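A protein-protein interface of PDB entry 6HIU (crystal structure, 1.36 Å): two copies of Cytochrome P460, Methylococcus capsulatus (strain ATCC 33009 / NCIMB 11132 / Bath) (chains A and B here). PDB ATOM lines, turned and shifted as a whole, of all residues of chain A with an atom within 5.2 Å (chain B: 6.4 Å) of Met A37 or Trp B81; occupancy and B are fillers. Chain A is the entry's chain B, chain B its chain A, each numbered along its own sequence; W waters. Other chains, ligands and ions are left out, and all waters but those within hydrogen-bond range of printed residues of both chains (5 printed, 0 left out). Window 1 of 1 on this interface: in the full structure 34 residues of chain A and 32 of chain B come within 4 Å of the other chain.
Positions printed for both chains: 35, 37 and 53.
Of the 13 printed residues of chain A, 7 touch a printed residue of chain B. Printed residues of chain A that touch a printed residue of chain B: Lys A36, Met A37, Val A40, Arg A63, Ala A158, Lys A159 and Leu A160. Of the 23 printed residues of chain B, 8 touch a printed residue of chain A. Among the printed residues, Asp or Glu carboxylates within 4 Å of a Lys or Arg side-chain nitrogen of the other chain: Arg A63 with Asp B34.
Water W5 bridges NZ of Lys A159 and OD1 of Asp B97. Water W1 lies within hydrogen-bond range of the backbone carbonyl oxygen (O) of Met A37, the backbone carbonyl oxygen (O) of Lys B33 and the guanidinium group (NH2) of Arg A63. Water W4 bridges the backbone carbonyl oxygen (O) of Trp A35 and the backbone NH (N) of Met B37. Water W3 lies within hydrogen-bond range of the backbone carbonyl oxygen of Trp B35 (2.8 Å), the backbone carbonyl oxygen of Lys B33 (2.8 Å) and the backbone NH of Met A37 (2.9 Å). Water W2 bridges O of Gly B96 and N of Lys A159.
Of the printed residues of chain B, Met A37 touches Trp B81 (3.9 Å). Printed residues of chain B within 4 Å of Lys A159: Trp B81 (2.9 Å), Gly B96 (3.7 Å) and Phe B98 (3.5 Å). Of the printed residues of chain A, Ala B51 touches Val A40 (3.9 Å). Leu B79 touches none of the printed residues of chain A. Of the printed residues of chain A, Trp B81 touches Met A37 (3.9 Å), Ala A158 (3.6 Å), Lys A159 (2.9 Å) and Leu A160 (3.9 Å). Printed residues of chain A within 4 Å of Pro B95: Val A40. The nearest printed residue of chain B that does not touch Met A37 is Leu B79 (4.4 Å). The nearest printed residue of chain A that does not touch Trp B81 is Val A40 (4.2 Å). The nearest printed residue of chain B that does not touch Lys A159 is Asp B97 (4.4 Å).
Lys A36 touches Asp B34 (CD to OD1, 3.7 Å). CE of Met A37 touches CH2 of Trp B81 (3.9 Å). Leu B49 touches Val A40. Ala B51 touches Val A40 (CB to CG1, 3.9 Å). Val A40 touches Pro B95 (O to CD, 3.2 Å). Ala A158 touches Trp B81. Phe B98 touches Lys A159 (CB to O, 3.5 Å). NZ of Lys B33 touches O of Leu A160, 3.9 Å away. Trp B81 touches Leu A160 (CZ2 to CD2, 3.9 Å). Leu A160 touches Phe B98.
NH1 of Arg A63 lies within salt-bridge range of OD1 of Asp B34 (2.8 Å). The guanidinium group (NH2) of Arg A63 lies within hydrogen-bond range of the backbone carbonyl oxygen (O) of Lys B33 (3.3 Å). NE1 of Trp B81 lies within hydrogen-bond range of O of Lys A159.
The side-chain sulfur (SD) of Met A37 is in hydrogen-bond range of the backbone NH (N) of Gly A39. The backbone carbonyl oxygen of Ala B51 sits at hydrogen-bond distance from the backbone NH of Leu B79. The backbone NH (N) of Ala A158 sits at hydrogen-bond distance from the backbone carbonyl oxygen (O) of Ile A38 (3.0 Å). The backbone NH (N) of Leu B49 lies within hydrogen-bond range of the backbone carbonyl oxygen (O) of Trp B81 (2.9 Å). The backbone NH (N) of Gly B96 is in hydrogen-bond range of the backbone carbonyl oxygen (O) of Lys B82 (2.8 Å).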
ATOM      1  N   TRP A  35     -12.287  14.442  16.789  1.00  0.00           N
ATOM      2  CA  TRP A  35     -10.991  14.857  16.268  1.00  0.00           C
ATOM      3  C   TRP A  35     -10.581  14.060  15.015  1.00  0.00           C
ATOM      4  O   TRP A  35     -10.933  12.905  14.854  1.00  0.00           O
ATOM      5  CB  TRP A  35      -9.902  14.801  17.361  1.00  0.00           C
ATOM      6  CG  TRP A  35     -10.038  15.794  18.485  1.00  0.00           C
ATOM      7  CD1 TRP A  35     -10.921  16.822  18.616  1.00  0.00           C
ATOM      8  CD2 TRP A  35      -9.207  15.846  19.660  1.00  0.00           C
ATOM      9  NE1 TRP A  35     -10.707  17.499  19.788  1.00  0.00           N
ATOM     10  CE2 TRP A  35      -9.642  16.931  20.454  1.00  0.00           C
ATOM     11  CE3 TRP A  35      -8.135  15.063  20.126  1.00  0.00           C
ATOM     12  CZ2 TRP A  35      -9.100  17.199  21.726  1.00  0.00           C
ATOM     13  CZ3 TRP A  35      -7.581  15.366  21.350  1.00  0.00           C
ATOM     14  CH2 TRP A  35      -8.039  16.427  22.128  1.00  0.00           C
ATOM     15  N   LYS A  36      -9.726  14.654  14.184  1.00  0.00           N
ATOM     16  CA  LYS A  36      -9.175  14.024  12.961  1.00  0.00           C
ATOM     17  C   LYS A  36      -8.124  12.953  13.292  1.00  0.00           C
ATOM     18  O   LYS A  36      -7.402  13.007  14.305  1.00  0.00           O
ATOM     19  CB  LYS A  36      -8.613  15.097  12.020  1.00  0.00           C
ATOM     20  CG  LYS A  36      -9.665  16.123  11.540  1.00  0.00           C
ATOM     21  CD  LYS A  36      -9.099  17.373  10.848  1.00  0.00           C
ATOM     22  CE  LYS A  36     -10.077  18.539  10.621  1.00  0.00           C
ATOM     23  NZ  LYS A  36     -10.835  18.968  11.821  1.00  0.00           N
ATOM     24  N   MET A  37      -8.069  11.976  12.386  1.00  0.00           N
ATOM     25  CA  MET A  37      -7.177  10.788  12.471  1.00  0.00           C
ATOM     26  C   MET A  37      -5.722  11.165  12.129  1.00  0.00           C
ATOM     27  O   MET A  37      -5.465  11.766  11.015  1.00  0.00           O
ATOM     28  CB  MET A  37      -7.700   9.728  11.486  1.00  0.00           C
ATOM     29  CG  MET A  37      -7.015   8.381  11.589  1.00  0.00           C
ATOM     30  SD  MET A  37      -5.520   8.165  10.622  1.00  0.00           S
ATOM     31  CE  MET A  37      -6.067   8.538   8.961  1.00  0.00           C
ATOM     32  N   ILE A  38      -4.779  10.789  12.994  1.00  0.00           N
ATOM     33  CA  ILE A  38      -3.339  10.824  12.720  1.00  0.00           C
ATOM     34  C   ILE A  38      -2.830   9.431  12.312  1.00  0.00           C
ATOM     35  O   ILE A  38      -2.040   9.314  11.358  1.00  0.00           O
ATOM     36  CB  ILE A  38      -2.582  11.418  13.905  1.00  0.00           C
ATOM     37  CG1 ILE A  38      -2.893  12.919  13.993  1.00  0.00           C
ATOM     38  CG2 ILE A  38      -1.082  11.162  13.723  1.00  0.00           C
ATOM     39  CD1 ILE A  38      -2.316  13.661  15.149  1.00  0.00           C
ATOM     40  N   GLY A  39      -3.279   8.359  12.989  1.00  0.00           N
ATOM     41  CA  GLY A  39      -2.873   6.989  12.585  1.00  0.00           C
ATOM     42  C   GLY A  39      -3.658   5.909  13.299  1.00  0.00           C
ATOM     43  O   GLY A  39      -4.685   6.204  13.965  1.00  0.00           O
ATOM     44  N   VAL A  40      -3.213   4.638  13.111  1.00  0.00           N
ATOM     45  CA  VAL A  40      -3.789   3.473  13.758  1.00  0.00           C
ATOM     46  C   VAL A  40      -2.634   2.536  14.175  1.00  0.00           C
ATOM     47  O   VAL A  40      -1.550   2.657  13.626  1.00  0.00           O
ATOM     48  CB  VAL A  40      -4.787   2.752  12.820  1.00  0.00           C
ATOM     49  CG1 VAL A  40      -6.009   3.605  12.464  1.00  0.00           C
ATOM     50  CG2 VAL A  40      -4.115   2.249  11.573  1.00  0.00           C
ATOM     51  N   ILE A  52      -5.212   6.661  16.761  1.00  0.00           N
ATOM     52  CA  ILE A  52      -4.497   7.833  17.217  1.00  0.00           C
ATOM     53  C   ILE A  52      -5.128   9.042  16.502  1.00  0.00           C
ATOM     54  O   ILE A  52      -5.082   9.150  15.270  1.00  0.00           O
ATOM     55  CB  ILE A  52      -2.952   7.795  16.997  1.00  0.00           C
ATOM     56  CG1 ILE A  52      -2.269   6.565  17.610  1.00  0.00           C
ATOM     57  CG2 ILE A  52      -2.350   9.064  17.556  1.00  0.00           C
ATOM     58  CD1 ILE A  52      -2.166   5.388  16.700  1.00  0.00           C
ATOM     59  N   LEU A  53      -5.784   9.900  17.318  1.00  0.00           N
ATOM     60  CA  LEU A  53      -6.370  11.180  16.835  1.00  0.00           C
ATOM     61  C   LEU A  53      -5.600  12.364  17.434  1.00  0.00           C
ATOM     62  O   LEU A  53      -4.817  12.204  18.369  1.00  0.00           O
ATOM     63  CB  LEU A  53      -7.848  11.279  17.243  1.00  0.00           C
ATOM     64  CG  LEU A  53      -8.765  10.031  17.084  1.00  0.00           C
ATOM     65  CD1 LEU A  53     -10.185  10.369  17.545  1.00  0.00           C
ATOM     66  CD2 LEU A  53      -8.744   9.489  15.652  1.00  0.00           C
ATOM     67  N   VAL A  59      -2.834  18.055  14.375  1.00  0.00           N
ATOM     68  CA  VAL A  59      -3.041  17.493  13.026  1.00  0.00           C
ATOM     69  C   VAL A  59      -2.263  18.325  11.982  1.00  0.00           C
ATOM     70  O   VAL A  59      -1.606  17.788  11.098  1.00  0.00           O
ATOM     71  CB  VAL A  59      -4.550  17.311  12.702  1.00  0.00           C
ATOM     72  CG1 VAL A  59      -4.794  17.066  11.217  1.00  0.00           C
ATOM     73  CG2 VAL A  59      -5.188  16.189  13.539  1.00  0.00           C
ATOM     74  N   ARG A  63       0.939  16.880   9.698  1.00  0.00           N
ATOM     75  CA  ARG A  63       0.883  16.847   8.252  1.00  0.00           C
ATOM     76  C   ARG A  63       2.034  17.687   7.678  1.00  0.00           C
ATOM     77  O   ARG A  63       2.477  17.430   6.552  1.00  0.00           O
ATOM     78  CB  ARG A  63      -0.486  17.325   7.764  1.00  0.00           C
ATOM     79  CG  ARG A  63      -1.593  16.326   8.056  1.00  0.00           C
ATOM     80  CD  ARG A  63      -2.967  16.895   7.800  1.00  0.00           C
ATOM     81  NE  ARG A  63      -4.025  15.942   8.051  1.00  0.00           N
ATOM     82  CZ  ARG A  63      -5.315  16.204   7.868  1.00  0.00           C
ATOM     83  NH1 ARG A  63      -5.728  17.393   7.429  1.00  0.00           N
ATOM     84  NH2 ARG A  63      -6.214  15.254   8.112  1.00  0.00           N
ATOM     85  N   ALA A 158       0.305   8.561   9.660  1.00  0.00           N
ATOM     86  CA  ALA A 158       0.031   7.707   8.497  1.00  0.00           C
ATOM     87  C   ALA A 158       0.002   8.538   7.206  1.00  0.00           C
ATOM     88  O   ALA A 158      -0.479   9.671   7.202  1.00  0.00           O
ATOM     89  CB  ALA A 158      -1.274   6.958   8.681  1.00  0.00           C
ATOM     90  N   LYS A 159       0.590   7.982   6.153  1.00  0.00           N
ATOM     91  CA  LYS A 159       0.698   8.641   4.840  1.00  0.00           C
ATOM     92  C   LYS A 159      -0.625   8.548   4.065  1.00  0.00           C
ATOM     93  O   LYS A 159      -1.195   7.457   3.874  1.00  0.00           O
ATOM     94  CB  LYS A 159       1.835   7.991   4.051  1.00  0.00           C
ATOM     95  CG  LYS A 159       3.226   8.294   4.589  1.00  0.00           C
ATOM     96  CD  LYS A 159       4.323   7.728   3.696  1.00  0.00           C
ATOM     97  CE  LYS A 159       4.326   6.215   3.615  1.00  0.00           C
ATOM     98  NZ  LYS A 159       4.955   5.616   4.817  1.00  0.00           N
ATOM     99  N   LEU A 160      -1.094   9.712   3.570  1.00  0.00           N
ATOM    100  CA  LEU A 160      -2.287   9.793   2.704  1.00  0.00           C
ATOM    101  C   LEU A 160      -2.034  10.801   1.588  1.00  0.00           C
ATOM    102  O   LEU A 160      -1.279  11.743   1.808  1.00  0.00           O
ATOM    103  CB  LEU A 160      -3.512  10.238   3.507  1.00  0.00           C
ATOM    104  CG  LEU A 160      -4.120   9.193   4.437  1.00  0.00           C
ATOM    105  CD1 LEU A 160      -5.159   9.846   5.331  1.00  0.00           C
ATOM    106  CD2 LEU A 160      -4.678   8.040   3.620  1.00  0.00           C
ATOM    107  N   LYS B  33      -9.989  12.787   4.195  1.00  0.00           N
ATOM    108  CA  LYS B  33      -9.013  12.589   5.252  1.00  0.00           C
ATOM    109  C   LYS B  33      -9.331  13.372   6.537  1.00  0.00           C
ATOM    110  O   LYS B  33      -8.696  13.069   7.586  1.00  0.00           O
ATOM    111  CB  LYS B  33      -7.614  12.922   4.726  1.00  0.00           C
ATOM    112  CG  LYS B  33      -7.294  14.402   4.646  1.00  0.00           C
ATOM    113  CD  LYS B  33      -5.776  14.688   4.472  1.00  0.00           C
ATOM    114  CE  LYS B  33      -5.199  14.120   3.203  1.00  0.00           C
ATOM    115  NZ  LYS B  33      -3.748  14.454   3.089  1.00  0.00           N
ATOM    116  N   ASP B  34     -10.290  14.338   6.520  1.00  0.00           N
ATOM    117  CA  ASP B  34     -10.699  15.120   7.665  1.00  0.00           C
ATOM    118  C   ASP B  34     -11.976  14.547   8.329  1.00  0.00           C
ATOM    119  O   ASP B  34     -12.506  15.165   9.244  1.00  0.00           O
ATOM    120  CB  ASP B  34     -10.885  16.591   7.263  1.00  0.00           C
ATOM    121  CG  ASP B  34      -9.590  17.307   6.854  1.00  0.00           C
ATOM    122  OD1 ASP B  34      -8.503  16.877   7.275  1.00  0.00           O
ATOM    123  OD2 ASP B  34      -9.680  18.272   6.035  1.00  0.00           O
ATOM    124  N   TRP B  35     -12.501  13.420   7.831  1.00  0.00           N
ATOM    125  CA  TRP B  35     -13.757  12.878   8.341  1.00  0.00           C
ATOM    126  C   TRP B  35     -13.538  12.225   9.719  1.00  0.00           C
ATOM    127  O   TRP B  35     -12.455  11.718  10.000  1.00  0.00           O
ATOM    128  CB  TRP B  35     -14.335  11.860   7.367  1.00  0.00           C
ATOM    129  CG  TRP B  35     -14.873  12.432   6.081  1.00  0.00           C
ATOM    130  CD1 TRP B  35     -15.032  13.748   5.756  1.00  0.00           C
ATOM    131  CD2 TRP B  35     -15.452  11.676   5.001  1.00  0.00           C
ATOM    132  NE1 TRP B  35     -15.603  13.839   4.507  1.00  0.00           N
ATOM    133  CE2 TRP B  35     -15.880  12.597   4.018  1.00  0.00           C
ATOM    134  CE3 TRP B  35     -15.591  10.310   4.716  1.00  0.00           C
ATOM    135  CZ2 TRP B  35     -16.478  12.199   2.814  1.00  0.00           C
ATOM    136  CZ3 TRP B  35     -16.157   9.919   3.521  1.00  0.00           C
ATOM    137  CH2 TRP B  35     -16.594  10.854   2.585  1.00  0.00           C
ATOM    138  N   MET B  37     -13.871   9.448  12.823  1.00  0.00           N
ATOM    139  CA  MET B  37     -13.586   8.019  12.971  1.00  0.00           C
ATOM    140  C   MET B  37     -14.861   7.258  13.374  1.00  0.00           C
ATOM    141  O   MET B  37     -15.583   7.643  14.341  1.00  0.00           O
ATOM    142  CB  MET B  37     -12.470   7.818  14.013  1.00  0.00           C
ATOM    143  CG  MET B  37     -11.999   6.369  14.207  1.00  0.00           C
ATOM    144  SD  MET B  37     -12.943   5.341  15.362  1.00  0.00           S
ATOM    145  CE  MET B  37     -12.826   6.340  16.847  1.00  0.00           C
ATOM    146  N   GLN B  46      -4.533 -10.090   4.521  1.00  0.00           N
ATOM    147  CA  GLN B  46      -4.067  -8.965   3.679  1.00  0.00           C
ATOM    148  C   GLN B  46      -2.822  -8.292   4.274  1.00  0.00           C
ATOM    149  O   GLN B  46      -2.235  -7.442   3.625  1.00  0.00           O
ATOM    150  CB  GLN B  46      -5.180  -7.917   3.530  1.00  0.00           C
ATOM    151  CG  GLN B  46      -6.390  -8.424   2.767  1.00  0.00           C
ATOM    152  CD  GLN B  46      -7.488  -7.390   2.624  1.00  0.00           C
ATOM    153  OE1 GLN B  46      -7.537  -6.366   3.319  1.00  0.00           O
ATOM    154  NE2 GLN B  46      -8.376  -7.642   1.680  1.00  0.00           N
ATOM    155  N   ASN B  47      -2.434  -8.639   5.504  1.00  0.00           N
ATOM    156  CA  ASN B  47      -1.301  -8.089   6.182  1.00  0.00           C
ATOM    157  C   ASN B  47      -1.401  -6.555   6.244  1.00  0.00           C
ATOM    158  O   ASN B  47      -0.425  -5.847   5.956  1.00  0.00           O
ATOM    159  CB  ASN B  47      -0.009  -8.550   5.498  1.00  0.00           C
ATOM    160  CG  ASN B  47       1.212  -8.220   6.319  1.00  0.00           C
ATOM    161  OD1 ASN B  47       1.204  -8.335   7.543  1.00  0.00           O
ATOM    162  ND2 ASN B  47       2.267  -7.804   5.636  1.00  0.00           N
ATOM    163  N   ASN B  48      -2.574  -6.042   6.657  1.00  0.00           N
ATOM    164  CA  ASN B  48      -2.804  -4.583   6.606  1.00  0.00           C
ATOM    165  C   ASN B  48      -3.469  -4.090   7.895  1.00  0.00           C
ATOM    166  O   ASN B  48      -3.887  -4.859   8.765  1.00  0.00           O
ATOM    167  CB  ASN B  48      -3.670  -4.201   5.398  1.00  0.00           C
ATOM    168  CG  ASN B  48      -5.100  -4.661   5.526  1.00  0.00           C
ATOM    169  OD1 ASN B  48      -5.478  -5.264   6.538  1.00  0.00           O
ATOM    170  ND2 ASN B  48      -5.917  -4.351   4.532  1.00  0.00           N
ATOM    171  N   LEU B  49      -3.414  -2.778   8.063  1.00  0.00           N
ATOM    172  CA  LEU B  49      -4.137  -2.051   9.089  1.00  0.00           C
ATOM    173  C   LEU B  49      -5.139  -1.140   8.381  1.00  0.00           C
ATOM    174  O   LEU B  49      -4.799  -0.583   7.302  1.00  0.00           O
ATOM    175  CB  LEU B  49      -3.171  -1.196   9.906  1.00  0.00           C
ATOM    176  CG  LEU B  49      -2.175  -1.945  10.800  1.00  0.00           C
ATOM    177  CD1 LEU B  49      -1.088  -0.996  11.263  1.00  0.00           C
ATOM    178  CD2 LEU B  49      -2.828  -2.651  11.974  1.00  0.00           C
ATOM    179  N   ARG B  50      -6.335  -0.930   8.976  1.00  0.00           N
ATOM    180  CA  ARG B  50      -7.369  -0.089   8.328  1.00  0.00           C
ATOM    181  C   ARG B  50      -8.027   0.874   9.307  1.00  0.00           C
ATOM    182  O   ARG B  50      -8.207   0.552  10.515  1.00  0.00           O
ATOM    183  CB  ARG B  50      -8.431  -0.982   7.684  1.00  0.00           C
ATOM    184  CG  ARG B  50      -7.862  -2.107   6.838  1.00  0.00           C
ATOM    185  CD  ARG B  50      -8.884  -2.901   6.075  1.00  0.00           C
ATOM    186  NE  ARG B  50      -9.327  -2.218   4.870  1.00  0.00           N
ATOM    187  CZ  ARG B  50     -10.193  -2.737   3.985  1.00  0.00           C
ATOM    188  NH1 ARG B  50     -10.676  -3.952   4.201  1.00  0.00           N
ATOM    189  NH2 ARG B  50     -10.560  -2.049   2.902  1.00  0.00           N
ATOM    190  N   ALA B  51      -8.370   2.069   8.789  1.00  0.00           N
ATOM    191  CA  ALA B  51      -9.215   3.026   9.492  1.00  0.00           C
ATOM    192  C   ALA B  51     -10.528   3.163   8.716  1.00  0.00           C
ATOM    193  O   ALA B  51     -10.526   3.177   7.467  1.00  0.00           O
ATOM    194  CB  ALA B  51      -8.524   4.341   9.610  1.00  0.00           C
ATOM    195  N   LEU B  53     -13.682   5.736   8.398  1.00  0.00           N
ATOM    196  CA  LEU B  53     -14.171   7.071   8.661  1.00  0.00           C
ATOM    197  C   LEU B  53     -15.545   7.233   7.974  1.00  0.00           C
ATOM    198  O   LEU B  53     -15.947   6.391   7.156  1.00  0.00           O
ATOM    199  CB  LEU B  53     -13.188   8.148   8.164  1.00  0.00           C
ATOM    200  CG  LEU B  53     -11.687   7.939   8.431  1.00  0.00           C
ATOM    201  CD1 LEU B  53     -10.900   9.108   7.872  1.00  0.00           C
ATOM    202  CD2 LEU B  53     -11.364   7.787   9.907  1.00  0.00           C
ATOM    203  N   LEU B  79      -9.642   3.128   4.754  1.00  0.00           N
ATOM    204  CA  LEU B  79      -8.242   3.438   4.360  1.00  0.00           C
ATOM    205  C   LEU B  79      -7.331   2.307   4.819  1.00  0.00           C
ATOM    206  O   LEU B  79      -7.429   1.905   5.985  1.00  0.00           O
ATOM    207  CB  LEU B  79      -7.857   4.778   4.987  1.00  0.00           C
ATOM    208  CG  LEU B  79      -8.759   5.988   4.694  1.00  0.00           C
ATOM    209  CD1 LEU B  79      -8.350   7.213   5.498  1.00  0.00           C
ATOM    210  CD2 LEU B  79      -8.759   6.260   3.183  1.00  0.00           C
ATOM    211  N   SER B  80      -6.501   1.760   3.911  1.00  0.00           N
ATOM    212  CA  SER B  80      -5.656   0.593   4.200  1.00  0.00           C
ATOM    213  C   SER B  80      -4.190   0.929   3.997  1.00  0.00           C
ATOM    214  O   SER B  80      -3.846   1.552   2.974  1.00  0.00           O
ATOM    215  CB  SER B  80      -6.011  -0.546   3.289  1.00  0.00           C
ATOM    216  OG  SER B  80      -7.377  -0.911   3.385  1.00  0.00           O
ATOM    217  N   TRP B  81      -3.355   0.471   4.927  1.00  0.00           N
ATOM    218  CA  TRP B  81      -1.881   0.517   4.849  1.00  0.00           C
ATOM    219  C   TRP B  81      -1.298  -0.875   5.094  1.00  0.00           C
ATOM    220  O   TRP B  81      -1.819  -1.643   5.876  1.00  0.00           O
ATOM    221  CB  TRP B  81      -1.311   1.471   5.889  1.00  0.00           C
ATOM    222  CG  TRP B  81      -1.783   2.885   5.824  1.00  0.00           C
ATOM    223  CD1 TRP B  81      -1.171   3.923   5.200  1.00  0.00           C
ATOM    224  CD2 TRP B  81      -2.961   3.444   6.460  1.00  0.00           C
ATOM    225  NE1 TRP B  81      -1.887   5.076   5.371  1.00  0.00           N
ATOM    226  CE2 TRP B  81      -2.976   4.827   6.173  1.00  0.00           C
ATOM    227  CE3 TRP B  81      -3.954   2.917   7.287  1.00  0.00           C
ATOM    228  CZ2 TRP B  81      -3.992   5.674   6.623  1.00  0.00           C
ATOM    229  CZ3 TRP B  81      -4.953   3.761   7.758  1.00  0.00           C
ATOM    230  CH2 TRP B  81      -4.961   5.119   7.436  1.00  0.00           C
ATOM    231  N   LYS B  82      -0.160  -1.149   4.430  1.00  0.00           N
ATOM    232  CA  LYS B  82       0.587  -2.369   4.749  1.00  0.00           C
ATOM    233  C   LYS B  82       1.073  -2.275   6.195  1.00  0.00           C
ATOM    234  O   LYS B  82       1.485  -1.219   6.651  1.00  0.00           O
ATOM    235  CB  LYS B  82       1.822  -2.474   3.841  1.00  0.00           C
ATOM    236  CG  LYS B  82       1.537  -2.520   2.359  1.00  0.00           C
ATOM    237  N   LYS B  83       1.081  -3.408   6.916  1.00  0.00           N
ATOM    238  CA  LYS B  83       1.673  -3.481   8.253  1.00  0.00           C
ATOM    239  C   LYS B  83       3.196  -3.300   8.182  1.00  0.00           C
ATOM    240  O   LYS B  83       3.882  -3.824   7.283  1.00  0.00           O
ATOM    241  CB  LYS B  83       1.437  -4.822   8.944  1.00  0.00           C
ATOM    242  CG  LYS B  83       0.059  -5.010   9.533  1.00  0.00           C
ATOM    243  CD  LYS B  83      -0.061  -6.231  10.426  1.00  0.00           C
ATOM    244  CE  LYS B  83      -1.467  -6.779  10.547  1.00  0.00           C
ATOM    245  NZ  LYS B  83      -1.475  -8.157  11.110  1.00  0.00           N
ATOM    246  N   VAL B  94       2.297  -0.962  12.846  1.00  0.00           N
ATOM    247  CA  VAL B  94       1.993   0.429  12.534  1.00  0.00           C
ATOM    248  C   VAL B  94       1.902   0.586  11.012  1.00  0.00           C
ATOM    249  O   VAL B  94       2.389  -0.258  10.239  1.00  0.00           O
ATOM    250  CB  VAL B  94       3.028   1.411  13.110  1.00  0.00           C
ATOM    251  CG1 VAL B  94       3.109   1.400  14.631  1.00  0.00           C
ATOM    252  CG2 VAL B  94       4.409   1.170  12.483  1.00  0.00           C
ATOM    253  N   PRO B  95       1.269   1.660  10.492  1.00  0.00           N
ATOM    254  CA  PRO B  95       1.140   1.810   9.047  1.00  0.00           C
ATOM    255  C   PRO B  95       2.465   1.996   8.299  1.00  0.00           C
ATOM    256  O   PRO B  95       3.315   2.822   8.685  1.00  0.00           O
ATOM    257  CB  PRO B  95       0.201   3.033   8.884  1.00  0.00           C
ATOM    258  CG  PRO B  95      -0.467   3.179  10.250  1.00  0.00           C
ATOM    259  CD  PRO B  95       0.580   2.729  11.238  1.00  0.00           C
ATOM    260  N   GLY B  96       2.587   1.256   7.205  1.00  0.00           N
ATOM    261  CA  GLY B  96       3.633   1.513   6.195  1.00  0.00           C
ATOM    262  C   GLY B  96       3.039   2.173   4.961  1.00  0.00           C
ATOM    263  O   GLY B  96       2.272   3.130   5.042  1.00  0.00           O
ATOM    264  N   ASP B  97       3.341   1.631   3.786  1.00  0.00           N
ATOM    265  CA  ASP B  97       2.859   2.200   2.522  1.00  0.00           C
ATOM    266  C   ASP B  97       1.316   2.188   2.494  1.00  0.00           C
ATOM    267  O   ASP B  97       0.677   1.167   2.839  1.00  0.00           O
ATOM    268  CB  ASP B  97       3.376   1.463   1.275  1.00  0.00           C
ATOM    269  CG  ASP B  97       4.876   1.564   1.022  1.00  0.00           C
ATOM    270  OD1 ASP B  97       5.541   2.460   1.596  1.00  0.00           O
ATOM    271  OD2 ASP B  97       5.357   0.704   0.266  1.00  0.00           O
ATOM    272  N   PHE B  98       0.757   3.273   1.954  1.00  0.00           N
ATOM    273  CA  PHE B  98      -0.710   3.409   1.715  1.00  0.00           C
ATOM    274  C   PHE B  98      -1.134   2.575   0.516  1.00  0.00           C
ATOM    275  O   PHE B  98      -0.533   2.698  -0.592  1.00  0.00           O
ATOM    276  CB  PHE B  98      -1.095   4.874   1.473  1.00  0.00           C
ATOM    277  CG  PHE B  98      -2.575   5.114   1.189  1.00  0.00           C
ATOM    278  CD1 PHE B  98      -3.539   4.762   2.132  1.00  0.00           C
ATOM    279  CD2 PHE B  98      -2.995   5.701  -0.005  1.00  0.00           C
ATOM    280  CE1 PHE B  98      -4.886   4.978   1.866  1.00  0.00           C
ATOM    281  CE2 PHE B  98      -4.337   5.947  -0.257  1.00  0.00           C
ATOM    282  CZ  PHE B  98      -5.280   5.572   0.682  1.00  0.00           C
ATOM    283  N   THR B  99      -2.161   1.734   0.664  1.00  0.00           N
ATOM    284  CA  THR B  99      -2.587   0.794  -0.374  1.00  0.00           C
ATOM    285  C   THR B  99      -3.841   1.261  -1.138  1.00  0.00           C
ATOM    286  O   THR B  99      -3.814   1.294  -2.368  1.00  0.00           O
ATOM    287  CB  THR B  99      -2.753  -0.654   0.121  1.00  0.00           C
ATOM    288  OG1 THR B  99      -3.859  -0.788   0.991  1.00  0.00           O
ATOM    289  CG2 THR B  99      -1.563  -1.148   0.899  1.00  0.00           C
ATOM    290  N   GLN B 100      -4.920   1.690  -0.454  1.00  0.00           N
ATOM    291  CA  GLN B 100      -6.158   2.032  -1.154  1.00  0.00           C
ATOM    292  C   GLN B 100      -7.148   2.743  -0.230  1.00  0.00           C
ATOM    293  O   GLN B 100      -7.119   2.609   1.026  1.00  0.00           O
ATOM    294  CB  GLN B 100      -6.847   0.810  -1.742  1.00  0.00           C
ATOM    295  CG  GLN B 100      -7.410  -0.147  -0.709  1.00  0.00           C
ATOM    296  CD  GLN B 100      -7.551  -1.580  -1.160  1.00  0.00           C
ATOM    297  OE1 GLN B 100      -6.674  -2.136  -1.821  1.00  0.00           O
ATOM    298  NE2 GLN B 100      -8.661  -2.194  -0.816  1.00  0.00           N
HETATM  299  O   HOH W   1      -6.173  12.254   8.428  1.00  0.00           O
HETATM  300  O   HOH W   2       2.107   5.454   6.550  1.00  0.00           O
HETATM  301  O   HOH W   3      -9.759  12.315  10.057  1.00  0.00           O
HETATM  302  O   HOH W   4     -13.181  11.326  14.907  1.00  0.00           O
HETATM  303  O   HOH W   5       6.020   3.321   4.177  1.00  0.00           O
